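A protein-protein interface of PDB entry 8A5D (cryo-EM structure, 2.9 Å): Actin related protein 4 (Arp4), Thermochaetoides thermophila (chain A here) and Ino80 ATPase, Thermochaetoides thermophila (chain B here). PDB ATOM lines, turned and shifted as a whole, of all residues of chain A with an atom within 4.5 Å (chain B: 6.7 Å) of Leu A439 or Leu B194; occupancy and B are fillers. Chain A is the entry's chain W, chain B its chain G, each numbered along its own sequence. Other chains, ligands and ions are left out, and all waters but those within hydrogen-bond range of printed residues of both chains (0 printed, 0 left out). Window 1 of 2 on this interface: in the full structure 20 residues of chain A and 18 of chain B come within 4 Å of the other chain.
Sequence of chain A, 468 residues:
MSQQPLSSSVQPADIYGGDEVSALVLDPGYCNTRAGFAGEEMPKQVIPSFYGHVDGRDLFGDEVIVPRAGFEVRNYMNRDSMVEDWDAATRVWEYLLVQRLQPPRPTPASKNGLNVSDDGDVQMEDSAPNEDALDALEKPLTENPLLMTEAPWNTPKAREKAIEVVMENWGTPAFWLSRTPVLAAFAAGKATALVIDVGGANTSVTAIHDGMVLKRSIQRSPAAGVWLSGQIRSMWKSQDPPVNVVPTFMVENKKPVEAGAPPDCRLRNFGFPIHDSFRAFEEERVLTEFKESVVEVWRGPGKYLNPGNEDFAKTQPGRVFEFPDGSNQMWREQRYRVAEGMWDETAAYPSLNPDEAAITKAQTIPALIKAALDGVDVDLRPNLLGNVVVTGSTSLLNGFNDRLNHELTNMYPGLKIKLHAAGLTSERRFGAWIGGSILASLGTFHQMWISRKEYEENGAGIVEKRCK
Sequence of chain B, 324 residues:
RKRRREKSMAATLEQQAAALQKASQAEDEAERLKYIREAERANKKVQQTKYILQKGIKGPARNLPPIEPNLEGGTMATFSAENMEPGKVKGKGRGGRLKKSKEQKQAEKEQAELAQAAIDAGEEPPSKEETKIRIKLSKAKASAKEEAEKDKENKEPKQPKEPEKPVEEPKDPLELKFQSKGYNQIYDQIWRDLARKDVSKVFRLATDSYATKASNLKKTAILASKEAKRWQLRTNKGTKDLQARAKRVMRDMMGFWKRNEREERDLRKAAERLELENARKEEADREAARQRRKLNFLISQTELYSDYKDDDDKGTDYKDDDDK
The side-chain carboxylate (OD2) of Asp B198 sits at hydrogen-bond distance from the side-chain hydroxyl (OG1) of Thr A444.
The backbone NH of Val B199 lies within hydrogen-bond range of the backbone carbonyl oxygen of Leu B194 (3.0 Å).
Trp B191 touches Phe A186. Phe A186 touches Val B199 (CG to CG2, 3.8 Å). Leu B194 touches Leu A439 (CD2 to CD1, 3.7 Å). Leu B194 touches Leu A442. Asp B198 touches Leu A442 (CB to CD1, 3.9 Å). Leu A442 touches Val B199 (CD1 to CG2, 3.8 Å). Leu B194 touches Thr A444. CD1 of Leu B194 touches N of Phe A445 (3.99 Å).
Of chain B, only Leu B194 comes within 4 Å of Leu A439. Ser A441 touches none of the printed residues of chain B. Printed residues of chain B within 4 Å of Phe A445: Leu B194. Printed residues of chain A within 4 Å of Trp B191: Phe A186. Of the printed residues of chain A, Asp B198 touches Leu A442 (3.9 Å) and Thr A444 (3.0 Å). Of the printed residues of chain A, Val B199 touches Phe A186 (3.8 Å) and Leu A442 (3.8 Å). The nearest printed residue of chain B that does not touch Phe A445 is Trp B191 (4.05 Å).
Hydrophobic or aromatic side chains of chain A that line the printed part of chain B: Phe A186, Leu A439 and Leu A442. Among the printed residues, 9 pairs touch across the chains. Among the printed residues, no Asp or Glu carboxylate lies within 4 Å of a Lys or Arg side-chain nitrogen of the other chain.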
ATOM      1  N   LEU A 147       5.615  -3.766 -29.988  1.00  0.00           N
ATOM      2  CA  LEU A 147       4.145  -3.719 -30.203  1.00  0.00           C
ATOM      3  C   LEU A 147       3.787  -4.550 -31.420  1.00  0.00           C
ATOM      4  O   LEU A 147       4.226  -4.206 -32.483  1.00  0.00           O
ATOM      5  CB  LEU A 147       3.651  -2.300 -30.434  1.00  0.00           C
ATOM      6  CG  LEU A 147       2.120  -2.202 -30.416  1.00  0.00           C
ATOM      7  CD1 LEU A 147       1.616  -1.089 -29.557  1.00  0.00           C
ATOM      8  CD2 LEU A 147       1.563  -2.011 -31.783  1.00  0.00           C
ATOM      9  N   LEU A 183      -6.184  -0.485 -34.148  1.00  0.00           N
ATOM     10  CA  LEU A 183      -5.088   0.314 -34.729  1.00  0.00           C
ATOM     11  C   LEU A 183      -5.629   1.073 -35.956  1.00  0.00           C
ATOM     12  O   LEU A 183      -5.352   2.299 -36.046  1.00  0.00           O
ATOM     13  CB  LEU A 183      -3.924  -0.617 -35.038  1.00  0.00           C
ATOM     14  CG  LEU A 183      -3.321  -1.293 -33.800  1.00  0.00           C
ATOM     15  CD1 LEU A 183      -2.051  -2.023 -34.149  1.00  0.00           C
ATOM     16  CD2 LEU A 183      -3.059  -0.318 -32.656  1.00  0.00           C
ATOM     17  N   PHE A 186      -7.516   4.140 -34.706  1.00  0.00           N
ATOM     18  CA  PHE A 186      -6.600   5.211 -34.213  1.00  0.00           C
ATOM     19  C   PHE A 186      -5.825   5.857 -35.385  1.00  0.00           C
ATOM     20  O   PHE A 186      -5.583   7.066 -35.350  1.00  0.00           O
ATOM     21  CB  PHE A 186      -5.596   4.703 -33.199  1.00  0.00           C
ATOM     22  CG  PHE A 186      -6.146   4.209 -31.907  1.00  0.00           C
ATOM     23  CD1 PHE A 186      -7.461   4.421 -31.551  1.00  0.00           C
ATOM     24  CD2 PHE A 186      -5.299   3.582 -31.016  1.00  0.00           C
ATOM     25  CE1 PHE A 186      -7.929   3.992 -30.328  1.00  0.00           C
ATOM     26  CE2 PHE A 186      -5.770   3.160 -29.795  1.00  0.00           C
ATOM     27  CZ  PHE A 186      -7.086   3.355 -29.463  1.00  0.00           C
ATOM     28  N   GLY A 435      -1.440   3.063 -36.886  1.00  0.00           N
ATOM     29  CA  GLY A 435      -2.149   3.109 -35.601  1.00  0.00           C
ATOM     30  C   GLY A 435      -1.231   2.657 -34.485  1.00  0.00           C
ATOM     31  O   GLY A 435      -1.221   3.312 -33.427  1.00  0.00           O
ATOM     32  N   GLY A 436      -0.505   1.557 -34.686  1.00  0.00           N
ATOM     33  CA  GLY A 436       0.542   1.087 -33.739  1.00  0.00           C
ATOM     34  C   GLY A 436       1.580   2.193 -33.489  1.00  0.00           C
ATOM     35  O   GLY A 436       1.952   2.443 -32.348  1.00  0.00           O
ATOM     36  N   SER A 437       2.026   2.855 -34.539  1.00  0.00           N
ATOM     37  CA  SER A 437       2.984   3.958 -34.477  1.00  0.00           C
ATOM     38  C   SER A 437       2.441   5.097 -33.622  1.00  0.00           C
ATOM     39  O   SER A 437       3.199   5.650 -32.833  1.00  0.00           O
ATOM     40  CB  SER A 437       3.377   4.403 -35.870  1.00  0.00           C
ATOM     41  OG  SER A 437       4.257   5.529 -35.856  1.00  0.00           O
ATOM     42  N   ILE A 438       1.201   5.499 -33.798  1.00  0.00           N
ATOM     43  CA  ILE A 438       0.585   6.599 -32.971  1.00  0.00           C
ATOM     44  C   ILE A 438       0.408   6.110 -31.518  1.00  0.00           C
ATOM     45  O   ILE A 438       0.920   6.763 -30.635  1.00  0.00           O
ATOM     46  CB  ILE A 438      -0.759   7.044 -33.564  1.00  0.00           C
ATOM     47  CG1 ILE A 438      -0.579   7.690 -34.931  1.00  0.00           C
ATOM     48  CG2 ILE A 438      -1.423   7.969 -32.579  1.00  0.00           C
ATOM     49  CD1 ILE A 438      -1.830   7.822 -35.708  1.00  0.00           C
ATOM     50  N   LEU A 439      -0.206   4.937 -31.319  1.00  0.00           N
ATOM     51  CA  LEU A 439      -0.434   4.329 -29.991  1.00  0.00           C
ATOM     52  C   LEU A 439       0.881   4.288 -29.203  1.00  0.00           C
ATOM     53  O   LEU A 439       0.929   4.822 -28.080  1.00  0.00           O
ATOM     54  CB  LEU A 439      -1.034   2.922 -30.172  1.00  0.00           C
ATOM     55  CG  LEU A 439      -1.218   2.115 -28.875  1.00  0.00           C
ATOM     56  CD1 LEU A 439      -2.157   2.878 -27.933  1.00  0.00           C
ATOM     57  CD2 LEU A 439      -1.728   0.710 -29.141  1.00  0.00           C
ATOM     58  N   ALA A 440       1.898   3.614 -29.713  1.00  0.00           N
ATOM     59  CA  ALA A 440       3.148   3.379 -28.959  1.00  0.00           C
ATOM     60  C   ALA A 440       3.919   4.691 -28.776  1.00  0.00           C
ATOM     61  O   ALA A 440       5.005   4.628 -28.199  1.00  0.00           O
ATOM     62  CB  ALA A 440       3.974   2.323 -29.651  1.00  0.00           C
ATOM     63  N   SER A 441       3.420   5.826 -29.258  1.00  0.00           N
ATOM     64  CA  SER A 441       4.051   7.147 -29.039  1.00  0.00           C
ATOM     65  C   SER A 441       3.274   8.022 -28.033  1.00  0.00           C
ATOM     66  O   SER A 441       3.767   9.132 -27.734  1.00  0.00           O
ATOM     67  CB  SER A 441       4.205   7.838 -30.356  1.00  0.00           C
ATOM     68  OG  SER A 441       2.983   8.449 -30.724  1.00  0.00           O
ATOM     69  N   LEU A 442       2.151   7.536 -27.479  1.00  0.00           N
ATOM     70  CA  LEU A 442       1.331   8.245 -26.450  1.00  0.00           C
ATOM     71  C   LEU A 442       1.918   8.018 -25.053  1.00  0.00           C
ATOM     72  O   LEU A 442       2.249   6.864 -24.682  1.00  0.00           O
ATOM     73  CB  LEU A 442      -0.112   7.748 -26.465  1.00  0.00           C
ATOM     74  CG  LEU A 442      -0.808   7.907 -27.797  1.00  0.00           C
ATOM     75  CD1 LEU A 442      -2.250   7.480 -27.694  1.00  0.00           C
ATOM     76  CD2 LEU A 442      -0.675   9.350 -28.248  1.00  0.00           C
ATOM     77  N   THR A 444       0.548   8.270 -22.140  1.00  0.00           N
ATOM     78  CA  THR A 444      -0.424   7.527 -21.296  1.00  0.00           C
ATOM     79  C   THR A 444      -0.337   6.021 -21.570  1.00  0.00           C
ATOM     80  O   THR A 444      -0.769   5.247 -20.719  1.00  0.00           O
ATOM     81  CB  THR A 444      -1.818   8.101 -21.498  1.00  0.00           C
ATOM     82  OG1 THR A 444      -1.695   9.467 -21.093  1.00  0.00           O
ATOM     83  CG2 THR A 444      -2.892   7.405 -20.691  1.00  0.00           C
ATOM     84  N   PHE A 445       0.215   5.614 -22.695  1.00  0.00           N
ATOM     85  CA  PHE A 445       0.222   4.196 -23.108  1.00  0.00           C
ATOM     86  C   PHE A 445       1.311   3.473 -22.326  1.00  0.00           C
ATOM     87  O   PHE A 445       1.173   2.265 -22.125  1.00  0.00           O
ATOM     88  CB  PHE A 445       0.347   4.052 -24.637  1.00  0.00           C
ATOM     89  CG  PHE A 445       0.423   2.621 -25.081  1.00  0.00           C
ATOM     90  CD1 PHE A 445      -0.675   1.788 -25.039  1.00  0.00           C
ATOM     91  CD2 PHE A 445       1.608   2.082 -25.519  1.00  0.00           C
ATOM     92  CE1 PHE A 445      -0.580   0.437 -25.372  1.00  0.00           C
ATOM     93  CE2 PHE A 445       1.715   0.730 -25.847  1.00  0.00           C
ATOM     94  CZ  PHE A 445       0.623  -0.094 -25.766  1.00  0.00           C
ATOM     95  N   GLN B 189     -11.059   2.663 -18.000  1.00  0.00           N
ATOM     96  CA  GLN B 189     -11.007   4.137 -17.802  1.00  0.00           C
ATOM     97  C   GLN B 189      -9.742   4.694 -18.463  1.00  0.00           C
ATOM     98  O   GLN B 189      -9.809   5.789 -19.037  1.00  0.00           O
ATOM     99  CB  GLN B 189     -11.081   4.436 -16.303  1.00  0.00           C
ATOM    100  CG  GLN B 189     -11.030   5.921 -15.953  1.00  0.00           C
ATOM    101  CD  GLN B 189     -11.042   6.177 -14.459  1.00  0.00           C
ATOM    102  OE1 GLN B 189     -11.517   5.361 -13.667  1.00  0.00           O
ATOM    103  NE2 GLN B 189     -10.511   7.323 -14.056  1.00  0.00           N
ATOM    104  N   ILE B 190      -8.625   3.972 -18.383  1.00  0.00           N
ATOM    105  CA  ILE B 190      -7.359   4.317 -19.099  1.00  0.00           C
ATOM    106  C   ILE B 190      -7.598   4.294 -20.616  1.00  0.00           C
ATOM    107  O   ILE B 190      -7.331   5.309 -21.270  1.00  0.00           O
ATOM    108  CB  ILE B 190      -6.217   3.407 -18.643  1.00  0.00           C
ATOM    109  CG1 ILE B 190      -5.799   3.825 -17.226  1.00  0.00           C
ATOM    110  CG2 ILE B 190      -5.054   3.461 -19.602  1.00  0.00           C
ATOM    111  CD1 ILE B 190      -4.809   2.883 -16.538  1.00  0.00           C
ATOM    112  N   TRP B 191      -8.160   3.234 -21.150  1.00  0.00           N
ATOM    113  CA  TRP B 191      -8.399   3.147 -22.605  1.00  0.00           C
ATOM    114  C   TRP B 191      -9.411   4.202 -23.069  1.00  0.00           C
ATOM    115  O   TRP B 191      -9.238   4.708 -24.187  1.00  0.00           O
ATOM    116  CB  TRP B 191      -8.770   1.717 -23.033  1.00  0.00           C
ATOM    117  CG  TRP B 191      -7.513   0.956 -23.205  1.00  0.00           C
ATOM    118  CD1 TRP B 191      -6.770   0.368 -22.220  1.00  0.00           C
ATOM    119  CD2 TRP B 191      -6.725   0.890 -24.404  1.00  0.00           C
ATOM    120  NE1 TRP B 191      -5.612  -0.139 -22.742  1.00  0.00           N
ATOM    121  CE2 TRP B 191      -5.544   0.187 -24.070  1.00  0.00           C
ATOM    122  CE3 TRP B 191      -6.940   1.272 -25.730  1.00  0.00           C
ATOM    123  CZ2 TRP B 191      -4.574  -0.122 -25.013  1.00  0.00           C
ATOM    124  CZ3 TRP B 191      -5.977   0.960 -26.664  1.00  0.00           C
ATOM    125  CH2 TRP B 191      -4.808   0.289 -26.304  1.00  0.00           C
ATOM    126  N   ARG B 192     -10.438   4.500 -22.298  1.00  0.00           N
ATOM    127  CA  ARG B 192     -11.422   5.521 -22.695  1.00  0.00           C
ATOM    128  C   ARG B 192     -10.702   6.870 -22.846  1.00  0.00           C
ATOM    129  O   ARG B 192     -10.939   7.558 -23.864  1.00  0.00           O
ATOM    130  CB  ARG B 192     -12.552   5.576 -21.678  1.00  0.00           C
ATOM    131  CG  ARG B 192     -13.520   6.746 -21.840  1.00  0.00           C
ATOM    132  CD  ARG B 192     -14.688   6.651 -20.869  1.00  0.00           C
ATOM    133  NE  ARG B 192     -15.400   5.395 -21.098  1.00  0.00           N
ATOM    134  CZ  ARG B 192     -15.517   4.372 -20.228  1.00  0.00           C
ATOM    135  NH1 ARG B 192     -15.019   4.439 -18.995  1.00  0.00           N
ATOM    136  NH2 ARG B 192     -16.143   3.271 -20.620  1.00  0.00           N
ATOM    137  N   ASP B 193      -9.881   7.268 -21.880  1.00  0.00           N
ATOM    138  CA  ASP B 193      -9.186   8.579 -21.925  1.00  0.00           C
ATOM    139  C   ASP B 193      -8.155   8.568 -23.056  1.00  0.00           C
ATOM    140  O   ASP B 193      -8.067   9.569 -23.770  1.00  0.00           O
ATOM    141  CB  ASP B 193      -8.608   8.916 -20.551  1.00  0.00           C
ATOM    142  CG  ASP B 193      -9.667   9.351 -19.539  1.00  0.00           C
ATOM    143  OD1 ASP B 193     -10.841   9.551 -19.943  1.00  0.00           O
ATOM    144  OD2 ASP B 193      -9.309   9.516 -18.349  1.00  0.00           O
ATOM    145  N   LEU B 194      -7.402   7.481 -23.199  1.00  0.00           N
ATOM    146  CA  LEU B 194      -6.395   7.304 -24.278  1.00  0.00           C
ATOM    147  C   LEU B 194      -7.020   7.450 -25.654  1.00  0.00           C
ATOM    148  O   LEU B 194      -6.501   8.220 -26.458  1.00  0.00           O
ATOM    149  CB  LEU B 194      -5.845   5.896 -24.217  1.00  0.00           C
ATOM    150  CG  LEU B 194      -4.553   5.695 -24.955  1.00  0.00           C
ATOM    151  CD1 LEU B 194      -3.456   6.285 -24.106  1.00  0.00           C
ATOM    152  CD2 LEU B 194      -4.305   4.228 -25.177  1.00  0.00           C
ATOM    153  N   ALA B 195      -8.123   6.758 -25.911  1.00  0.00           N
ATOM    154  CA  ALA B 195      -8.868   6.809 -27.193  1.00  0.00           C
ATOM    155  C   ALA B 195      -9.495   8.200 -27.409  1.00  0.00           C
ATOM    156  O   ALA B 195      -9.365   8.735 -28.534  1.00  0.00           O
ATOM    157  CB  ALA B 195      -9.908   5.711 -27.261  1.00  0.00           C
ATOM    158  N   ARG B 196     -10.192   8.772 -26.428  1.00  0.00           N
ATOM    159  CA  ARG B 196     -10.987  10.007 -26.664  1.00  0.00           C
ATOM    160  C   ARG B 196     -10.074  11.242 -26.669  1.00  0.00           C
ATOM    161  O   ARG B 196     -10.234  12.081 -27.582  1.00  0.00           O
ATOM    162  CB  ARG B 196     -12.123  10.119 -25.648  1.00  0.00           C
ATOM    163  CG  ARG B 196     -13.199   9.051 -25.791  1.00  0.00           C
ATOM    164  CD  ARG B 196     -14.380   9.391 -24.902  1.00  0.00           C
ATOM    165  NE  ARG B 196     -15.337   8.310 -24.671  1.00  0.00           N
ATOM    166  CZ  ARG B 196     -16.375   8.371 -23.831  1.00  0.00           C
ATOM    167  NH1 ARG B 196     -16.620   9.482 -23.149  1.00  0.00           N
ATOM    168  NH2 ARG B 196     -17.177   7.326 -23.680  1.00  0.00           N
ATOM    169  N   LYS B 197      -9.143  11.354 -25.720  1.00  0.00           N
ATOM    170  CA  LYS B 197      -8.331  12.589 -25.534  1.00  0.00           C
ATOM    171  C   LYS B 197      -7.015  12.498 -26.323  1.00  0.00           C
ATOM    172  O   LYS B 197      -6.762  13.394 -27.132  1.00  0.00           O
ATOM    173  CB  LYS B 197      -8.064  12.848 -24.051  1.00  0.00           C
ATOM    174  CG  LYS B 197      -9.298  13.004 -23.175  1.00  0.00           C
ATOM    175  CD  LYS B 197      -8.941  13.424 -21.757  1.00  0.00           C
ATOM    176  CE  LYS B 197     -10.115  13.927 -20.937  1.00  0.00           C
ATOM    177  NZ  LYS B 197      -9.671  14.568 -19.674  1.00  0.00           N
ATOM    178  N   ASP B 198      -6.184  11.489 -26.069  1.00  0.00           N
ATOM    179  CA  ASP B 198      -4.780  11.458 -26.557  1.00  0.00           C
ATOM    180  C   ASP B 198      -4.769  11.145 -28.060  1.00  0.00           C
ATOM    181  O   ASP B 198      -4.186  11.927 -28.809  1.00  0.00           O
ATOM    182  CB  ASP B 198      -3.916  10.470 -25.763  1.00  0.00           C
ATOM    183  CG  ASP B 198      -3.485  10.911 -24.368  1.00  0.00           C
ATOM    184  OD1 ASP B 198      -3.994  11.935 -23.854  1.00  0.00           O
ATOM    185  OD2 ASP B 198      -2.605  10.228 -23.805  1.00  0.00           O
ATOM    186  N   VAL B 199      -5.336  10.023 -28.498  1.00  0.00           N
ATOM    187  CA  VAL B 199      -5.375   9.642 -29.940  1.00  0.00           C
ATOM    188  C   VAL B 199      -5.918  10.789 -30.811  1.00  0.00           C
ATOM    189  O   VAL B 199      -5.275  11.049 -31.828  1.00  0.00           O
ATOM    190  CB  VAL B 199      -6.190   8.366 -30.166  1.00  0.00           C
ATOM    191  CG1 VAL B 199      -6.618   8.213 -31.622  1.00  0.00           C
ATOM    192  CG2 VAL B 199      -5.411   7.160 -29.708  1.00  0.00           C
ATOM    193  N   SER B 200      -6.977  11.490 -30.421  1.00  0.00           N
ATOM    194  CA  SER B 200      -7.526  12.606 -31.227  1.00  0.00           C
ATOM    195  C   SER B 200      -6.522  13.778 -31.321  1.00  0.00           C
ATOM    196  O   SER B 200      -6.397  14.347 -32.421  1.00  0.00           O
ATOM    197  CB  SER B 200      -8.877  13.054 -30.710  1.00  0.00           C
ATOM    198  OG  SER B 200      -8.792  13.610 -29.402  1.00  0.00           O
